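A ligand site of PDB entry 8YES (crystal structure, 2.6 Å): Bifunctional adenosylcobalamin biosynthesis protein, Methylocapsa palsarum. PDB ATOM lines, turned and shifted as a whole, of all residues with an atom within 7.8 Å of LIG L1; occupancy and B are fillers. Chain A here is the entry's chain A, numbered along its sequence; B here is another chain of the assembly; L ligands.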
ATOM      1  N   THR A  36       5.853  19.192  20.656  1.00  0.00           N
ATOM      2  CA  THR A  36       5.583  19.156  19.193  1.00  0.00           C
ATOM      3  C   THR A  36       4.107  19.423  18.905  1.00  0.00           C
ATOM      4  O   THR A  36       3.720  19.392  17.725  1.00  0.00           O
ATOM      5  CB  THR A  36       6.027  17.826  18.566  1.00  0.00           C
ATOM      6  OG1 THR A  36       5.285  16.783  19.165  1.00  0.00           O
ATOM      7  CG2 THR A  36       7.483  17.505  18.729  1.00  0.00           C
ATOM      8  N   ALA A  37       3.299  19.710  19.911  1.00  0.00           N
ATOM      9  CA  ALA A  37       1.895  20.147  19.709  1.00  0.00           C
ATOM     10  C   ALA A  37       1.398  20.906  20.947  1.00  0.00           C
ATOM     11  O   ALA A  37       1.844  20.560  22.047  1.00  0.00           O
ATOM     12  CB  ALA A  37       1.039  18.958  19.400  1.00  0.00           C
ATOM     13  N   GLN A  38       0.550  21.917  20.765  1.00  0.00           N
ATOM     14  CA  GLN A  38      -0.261  22.469  21.884  1.00  0.00           C
ATOM     15  C   GLN A  38      -1.570  21.683  21.845  1.00  0.00           C
ATOM     16  O   GLN A  38      -1.783  20.907  20.916  1.00  0.00           O
ATOM     17  CB  GLN A  38      -0.450  23.992  21.815  1.00  0.00           C
ATOM     18  CG  GLN A  38      -1.264  24.451  20.611  1.00  0.00           C
ATOM     19  CD  GLN A  38      -0.509  25.402  19.728  1.00  0.00           C
ATOM     20  OE1 GLN A  38       0.394  26.120  20.187  1.00  0.00           O
ATOM     21  NE2 GLN A  38      -0.857  25.419  18.450  1.00  0.00           N
ATOM     22  N   PRO A  39      -2.443  21.795  22.867  1.00  0.00           N
ATOM     23  CA  PRO A  39      -3.696  21.040  22.882  1.00  0.00           C
ATOM     24  C   PRO A  39      -4.832  21.903  22.346  1.00  0.00           C
ATOM     25  O   PRO A  39      -5.070  22.929  22.927  1.00  0.00           O
ATOM     26  CB  PRO A  39      -3.871  20.749  24.378  1.00  0.00           C
ATOM     27  CG  PRO A  39      -2.758  21.508  25.101  1.00  0.00           C
ATOM     28  CD  PRO A  39      -2.266  22.546  24.118  1.00  0.00           C
ATOM     29  N   LEU A  40      -5.513  21.447  21.292  1.00  0.00           N
ATOM     30  CA  LEU A  40      -6.600  22.195  20.593  1.00  0.00           C
ATOM     31  C   LEU A  40      -7.976  21.573  20.863  1.00  0.00           C
ATOM     32  O   LEU A  40      -8.975  22.064  20.298  1.00  0.00           O
ATOM     33  CB  LEU A  40      -6.263  22.211  19.100  1.00  0.00           C
ATOM     34  CG  LEU A  40      -4.890  22.783  18.745  1.00  0.00           C
ATOM     35  CD1 LEU A  40      -4.604  22.676  17.262  1.00  0.00           C
ATOM     36  CD2 LEU A  40      -4.756  24.238  19.209  1.00  0.00           C
ATOM     37  N   ASP A  41      -8.076  20.517  21.668  1.00  0.00           N
ATOM     38  CA  ASP A  41      -9.382  20.035  22.181  1.00  0.00           C
ATOM     39  C   ASP A  41      -9.226  19.760  23.671  1.00  0.00           C
ATOM     40  O   ASP A  41      -8.081  19.843  24.181  1.00  0.00           O
ATOM     41  CB  ASP A  41      -9.916  18.837  21.403  1.00  0.00           C
ATOM     42  CG  ASP A  41      -8.974  17.639  21.322  1.00  0.00           C
ATOM     43  OD1 ASP A  41      -8.101  17.516  22.206  1.00  0.00           O
ATOM     44  OD2 ASP A  41      -9.115  16.831  20.360  1.00  0.00           O
ATOM     45  N   ALA A  42     -10.350  19.444  24.333  1.00  0.00           N
ATOM     46  CA  ALA A  42     -10.481  19.253  25.800  1.00  0.00           C
ATOM     47  C   ALA A  42      -9.638  18.057  26.258  1.00  0.00           C
ATOM     48  O   ALA A  42      -8.876  18.225  27.227  1.00  0.00           O
ATOM     49  CB  ALA A  42     -11.939  19.054  26.123  1.00  0.00           C
ATOM     50  N   GLU A  43      -9.784  16.913  25.582  1.00  0.00           N
ATOM     51  CA  GLU A  43      -9.059  15.648  25.913  1.00  0.00           C
ATOM     52  C   GLU A  43      -7.556  15.905  25.908  1.00  0.00           C
ATOM     53  O   GLU A  43      -6.873  15.481  26.832  1.00  0.00           O
ATOM     54  CB  GLU A  43      -9.341  14.510  24.924  1.00  0.00           C
ATOM     55  CG  GLU A  43     -10.775  14.418  24.447  1.00  0.00           C
ATOM     56  CD  GLU A  43     -11.157  13.087  23.810  1.00  0.00           C
ATOM     57  OE1 GLU A  43     -12.395  12.792  23.769  1.00  0.00           O
ATOM     58  OE2 GLU A  43     -10.230  12.335  23.336  1.00  0.00           O
ATOM     59  N   MET A  44      -7.061  16.571  24.868  1.00  0.00           N
ATOM     60  CA  MET A  44      -5.607  16.806  24.681  1.00  0.00           C
ATOM     61  C   MET A  44      -5.155  17.821  25.737  1.00  0.00           C
ATOM     62  O   MET A  44      -4.016  17.673  26.246  1.00  0.00           O
ATOM     63  CB  MET A  44      -5.320  17.322  23.268  1.00  0.00           C
ATOM     64  CG  MET A  44      -3.968  16.888  22.728  1.00  0.00           C
ATOM     65  SD  MET A  44      -4.056  15.323  21.816  1.00  0.00           S
ATOM     66  CE  MET A  44      -2.914  14.341  22.786  1.00  0.00           C
ATOM     67  N   ALA A  45      -6.001  18.813  26.046  1.00  0.00           N
ATOM     68  CA  ALA A  45      -5.720  19.886  27.032  1.00  0.00           C
ATOM     69  C   ALA A  45      -5.344  19.252  28.376  1.00  0.00           C
ATOM     70  O   ALA A  45      -4.442  19.784  29.054  1.00  0.00           O
ATOM     71  CB  ALA A  45      -6.911  20.802  27.177  1.00  0.00           C
ATOM     72  N   LEU A  89       2.992  13.524  16.730  1.00  0.00           N
ATOM     73  CA  LEU A  89       2.267  14.805  16.587  1.00  0.00           C
ATOM     74  C   LEU A  89       2.954  15.737  15.578  1.00  0.00           C
ATOM     75  O   LEU A  89       2.253  16.324  14.755  1.00  0.00           O
ATOM     76  CB  LEU A  89       2.110  15.425  17.971  1.00  0.00           C
ATOM     77  CG  LEU A  89       0.899  14.874  18.720  1.00  0.00           C
ATOM     78  CD1 LEU A  89       1.040  15.069  20.208  1.00  0.00           C
ATOM     79  CD2 LEU A  89      -0.357  15.554  18.225  1.00  0.00           C
ATOM     80  N   SER A  92       2.024  14.584  12.203  1.00  0.00           N
ATOM     81  CA  SER A  92       0.619  15.007  12.058  1.00  0.00           C
ATOM     82  C   SER A  92       0.521  16.485  11.641  1.00  0.00           C
ATOM     83  O   SER A  92      -0.273  16.820  10.709  1.00  0.00           O
ATOM     84  CB  SER A  92      -0.130  14.746  13.309  1.00  0.00           C
ATOM     85  OG  SER A  92      -1.496  14.687  13.024  1.00  0.00           O
ATOM     86  N   ASN A  93       1.321  17.359  12.266  1.00  0.00           N
ATOM     87  CA  ASN A  93       1.380  18.790  11.905  1.00  0.00           C
ATOM     88  C   ASN A  93       1.753  18.919  10.417  1.00  0.00           C
ATOM     89  O   ASN A  93       1.055  19.643   9.693  1.00  0.00           O
ATOM     90  CB  ASN A  93       2.315  19.530  12.861  1.00  0.00           C
ATOM     91  CG  ASN A  93       1.813  19.531  14.284  1.00  0.00           C
ATOM     92  OD1 ASN A  93       0.612  19.322  14.538  1.00  0.00           O
ATOM     93  ND2 ASN A  93       2.710  19.763  15.242  1.00  0.00           N
ATOM     94  N   LEU A  96      -1.072  17.373   7.845  1.00  0.00           N
ATOM     95  CA  LEU A  96      -2.290  18.212   7.740  1.00  0.00           C
ATOM     96  C   LEU A  96      -1.966  19.525   7.019  1.00  0.00           C
ATOM     97  O   LEU A  96      -2.825  19.987   6.277  1.00  0.00           O
ATOM     98  CB  LEU A  96      -2.867  18.480   9.137  1.00  0.00           C
ATOM     99  CG  LEU A  96      -3.510  17.266   9.794  1.00  0.00           C
ATOM    100  CD1 LEU A  96      -4.004  17.604  11.186  1.00  0.00           C
ATOM    101  CD2 LEU A  96      -4.649  16.710   8.941  1.00  0.00           C
ATOM    102  N   LEU A 136      -6.180   9.670   4.171  1.00  0.00           N
ATOM    103  CA  LEU A 136      -5.416  10.519   5.118  1.00  0.00           C
ATOM    104  C   LEU A 136      -4.687   9.608   6.127  1.00  0.00           C
ATOM    105  O   LEU A 136      -3.444   9.632   6.149  1.00  0.00           O
ATOM    106  CB  LEU A 136      -6.362  11.519   5.790  1.00  0.00           C
ATOM    107  CG  LEU A 136      -5.704  12.430   6.810  1.00  0.00           C
ATOM    108  CD1 LEU A 136      -4.590  13.239   6.165  1.00  0.00           C
ATOM    109  CD2 LEU A 136      -6.724  13.340   7.481  1.00  0.00           C
ATOM    110  N   VAL B 131      -5.423   6.240  15.637  1.00  0.00           N
ATOM    111  CA  VAL B 131      -6.331   6.790  16.694  1.00  0.00           C
ATOM    112  C   VAL B 131      -7.770   6.661  16.214  1.00  0.00           C
ATOM    113  O   VAL B 131      -8.104   7.082  15.122  1.00  0.00           O
ATOM    114  CB  VAL B 131      -6.019   8.237  17.066  1.00  0.00           C
ATOM    115  CG1 VAL B 131      -6.163   9.160  15.862  1.00  0.00           C
ATOM    116  CG2 VAL B 131      -6.898   8.700  18.232  1.00  0.00           C
HETATM  117  N1  LIG L   1      -5.250  18.850  19.222  1.00  0.00           N
HETATM  118  C1  LIG L   1      -6.532  18.625  18.885  1.00  0.00           C
HETATM  119  N2  LIG L   1      -7.063  18.448  17.681  1.00  0.00           N
HETATM  120  C2  LIG L   1      -6.105  18.529  16.729  1.00  0.00           C
HETATM  121  N3  LIG L   1      -6.291  18.392  15.381  1.00  0.00           N
HETATM  122  C3  LIG L   1      -5.036  18.479  14.811  1.00  0.00           C
HETATM  123  N4  LIG L   1      -4.099  18.731  15.690  1.00  0.00           N
HETATM  124  C4  LIG L   1      -4.755  18.750  16.909  1.00  0.00           C
HETATM  125  C5  LIG L   1      -4.317  18.948  18.236  1.00  0.00           C
HETATM  126  N5  LIG L   1      -3.038  19.165  18.577  1.00  0.00           N
HETATM  127  C6  LIG L   1      -7.579  18.065  14.793  1.00  0.00           C
HETATM  128  C7  LIG L   1      -7.870  18.497  13.361  1.00  0.00           C
HETATM  129  C8  LIG L   1      -7.374  17.290  12.559  1.00  0.00           C
HETATM  130  C9  LIG L   1      -7.850  16.146  13.448  1.00  0.00           C
HETATM  131  C10 LIG L   1      -7.177  14.798  13.294  1.00  0.00           C
HETATM  132  O1  LIG L   1      -7.614  16.656  14.776  1.00  0.00           O
HETATM  133  O2  LIG L   1      -9.261  18.701  13.291  1.00  0.00           O
HETATM  134  O3  LIG L   1      -8.009  17.233  11.296  1.00  0.00           O
HETATM  135 CO1  LG2 L   2      -7.328  12.933  14.226  1.00  0.00          CO
HETATM  136  N1  LG2 L   2      -8.818  13.148  15.292  1.00  0.00           N
HETATM  137  N2  LG2 L   2      -8.421  12.103  12.991  1.00  0.00           N
HETATM  138  N3  LG2 L   2      -5.741  12.391  13.502  1.00  0.00           N
HETATM  139  N4  LG2 L   2      -6.501  13.666  15.868  1.00  0.00           N
HETATM  140  C1  LG2 L   2      -8.698  13.032  16.737  1.00  0.00           C
HETATM  141  C2  LG2 L   2      -8.869  11.540  17.114  1.00  0.00           C
HETATM  142  C3  LG2 L   2      -9.851  13.963  17.185  1.00  0.00           C
HETATM  143  C4  LG2 L   2     -10.446  13.598  18.543  1.00  0.00           C
HETATM  144  C5  LG2 L   2      -9.432  15.404  17.243  1.00  0.00           C
HETATM  145  C6  LG2 L   2     -10.574  16.433  17.136  1.00  0.00           C
HETATM  146  O1  LG2 L   2     -11.189  16.786  18.078  1.00  0.00           O
HETATM  147  N5  LG2 L   2     -10.863  16.975  15.944  1.00  0.00           N
HETATM  148  C7  LG2 L   2     -10.886  13.787  16.058  1.00  0.00           C
HETATM  149  C8  LG2 L   2     -11.998  12.755  16.367  1.00  0.00           C
HETATM  150  C9  LG2 L   2     -13.379  13.419  16.423  1.00  0.00           C
HETATM  151  C10 LG2 L   2     -14.423  12.521  17.004  1.00  0.00           C
HETATM  152  O2  LG2 L   2     -15.510  12.404  16.528  1.00  0.00           O
HETATM  153  N6  LG2 L   2     -14.102  11.869  18.087  1.00  0.00           N
HETATM  154  C11 LG2 L   2      -9.993  13.413  14.920  1.00  0.00           C
HETATM  155  C12 LG2 L   2     -10.357  13.412  13.538  1.00  0.00           C
HETATM  156  C13 LG2 L   2     -11.486  14.328  13.218  1.00  0.00           C
HETATM  157  C14 LG2 L   2      -9.652  12.702  12.635  1.00  0.00           C
HETATM  158  C15 LG2 L   2      -9.997  12.403  11.184  1.00  0.00           C
HETATM  159  C16 LG2 L   2     -11.410  11.857  10.946  1.00  0.00           C
HETATM  160  C17 LG2 L   2      -9.633  13.665  10.393  1.00  0.00           C
HETATM  161  C18 LG2 L   2     -10.609  14.043   9.293  1.00  0.00           C
HETATM  162  O3  LG2 L   2     -10.529  13.462   8.178  1.00  0.00           O
HETATM  163  N7  LG2 L   2     -11.465  15.034   9.653  1.00  0.00           N
HETATM  164  C19 LG2 L   2      -9.015  11.324  10.831  1.00  0.00           C
HETATM  165  C20 LG2 L   2      -9.579   9.956  11.140  1.00  0.00           C
HETATM  166  C21 LG2 L   2      -8.634   8.836  10.813  1.00  0.00           C
HETATM  167  C22 LG2 L   2      -9.271   7.521  11.168  1.00  0.00           C
HETATM  168  O4  LG2 L   2      -9.561   6.747  10.282  1.00  0.00           O
HETATM  169  N8  LG2 L   2      -9.432   7.224  12.460  1.00  0.00           N
HETATM  170  C23 LG2 L   2      -7.921  11.745  11.759  1.00  0.00           C
HETATM  171  C24 LG2 L   2      -6.533  11.682  11.390  1.00  0.00           C
HETATM  172  C25 LG2 L   2      -5.591  11.956  12.247  1.00  0.00           C
HETATM  173  C26 LG2 L   2      -4.164  11.692  11.898  1.00  0.00           C
HETATM  174  C27 LG2 L   2      -3.695  12.885  11.104  1.00  0.00           C
HETATM  175  C28 LG2 L   2      -4.051  10.424  11.072  1.00  0.00           C
HETATM  176  C29 LG2 L   2      -3.542  11.568  13.296  1.00  0.00           C
HETATM  177  C30 LG2 L   2      -3.352  10.111  13.638  1.00  0.00           C
HETATM  178  C31 LG2 L   2      -2.429   9.862  14.795  1.00  0.00           C
HETATM  179  C32 LG2 L   2      -2.523   8.418  15.190  1.00  0.00           C
HETATM  180  O5  LG2 L   2      -3.063   7.606  14.469  1.00  0.00           O
HETATM  181  N9  LG2 L   2      -1.961   8.141  16.352  1.00  0.00           N
HETATM  182  C33 LG2 L   2      -4.595  12.309  14.103  1.00  0.00           C
HETATM  183  C34 LG2 L   2      -4.266  12.991  15.348  1.00  0.00           C
HETATM  184  C35 LG2 L   2      -2.830  13.432  15.499  1.00  0.00           C
HETATM  185  C36 LG2 L   2      -5.181  13.303  16.244  1.00  0.00           C
HETATM  186  C37 LG2 L   2      -5.030  13.450  17.744  1.00  0.00           C
HETATM  187  C38 LG2 L   2      -4.940  14.940  17.916  1.00  0.00           C
HETATM  188  C39 LG2 L   2      -3.881  12.776  18.512  1.00  0.00           C
HETATM  189  C40 LG2 L   2      -3.832  11.280  18.445  1.00  0.00           C
HETATM  190  C41 LG2 L   2      -2.469  10.758  18.602  1.00  0.00           C
HETATM  191  O6  LG2 L   2      -1.602  11.155  17.917  1.00  0.00           O
HETATM  192  N10 LG2 L   2      -2.190  10.020  19.614  1.00  0.00           N
HETATM  193  C42 LG2 L   2      -6.382  12.896  18.186  1.00  0.00           C
HETATM  194  C43 LG2 L   2      -6.719  12.845  19.725  1.00  0.00           C
HETATM  195  C44 LG2 L   2      -7.430  13.940  20.413  1.00  0.00           C
HETATM  196  O7  LG2 L   2      -8.367  13.718  21.136  1.00  0.00           O
HETATM  197  N11 LG2 L   2      -6.968  15.157  20.315  1.00  0.00           N
HETATM  198  C45 LG2 L   2      -7.257  13.310  17.003  1.00  0.00           C
HETATM  199  C46 LG2 L   2      -2.256  10.561  20.967  1.00  0.00           C
HETATM  200  C47 LG2 L   2      -0.826  10.295  21.529  1.00  0.00           C
HETATM  201  C48 LG2 L   2       0.171  11.446  21.293  1.00  0.00           C
HETATM  202  O8  LG2 L   2      -0.975   9.951  22.899  1.00  0.00           O
HETATM  203  O9  LG2 L   2      -0.928   7.984  24.495  1.00  0.00           O
HETATM  204  O10 LG2 L   2       1.275   9.063  23.581  1.00  0.00           O
HETATM  205  P1  LG2 L   2      -0.176   8.669  23.369  1.00  0.00           P
HETATM  206  O11 LG2 L   2      -0.358   7.767  22.077  1.00  0.00           O
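The backbone carbonyl oxygen (O) of Gln 38 sits at hydrogen-bond distance from a nitrogen (N5) of LIG L1, 3.2 Å away.
The backbone NH of Leu 40 lies within hydrogen-bond range of a nitrogen (N1) of LIG L1, 3.3 Å away.
OD2 of Asp 41 is in hydrogen-bond range of N11 of LG2 L2 (2.7 Å).
The side-chain sulfur (SD) of Met 44 sits at hydrogen-bond distance from a nitrogen (N11) of LG2 L2, at 3.3 Å.
O5 of LG2 L2 is in hydrogen-bond range of N of Val 131 of chain B, 3.0 Å away.
A nitrogen (N8) of LG2 L2 sits at hydrogen-bond distance from the backbone carbonyl oxygen (O) of Val 131 of chain B (3.0 Å).
An oxygen (O1) of LIG L1 sits close to a nitrogen (N5) of LG2 L2 (3.5 Å).
OD1 of Asp 41 sits close to N of Met 44.
OD2 of Asp 41 touches C1 of LIG L1, 3.5 Å away.
Leu 96 touches LIG L1.
Hydrophobic or aromatic side chains that line LIG L1: Leu 40 and Leu 96.
Of the 16 residues printed, 4 come within 4 Å of LIG L1.
The nearest printed residue that does not touch LIG L1 is Ala 37 (4.2 Å).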
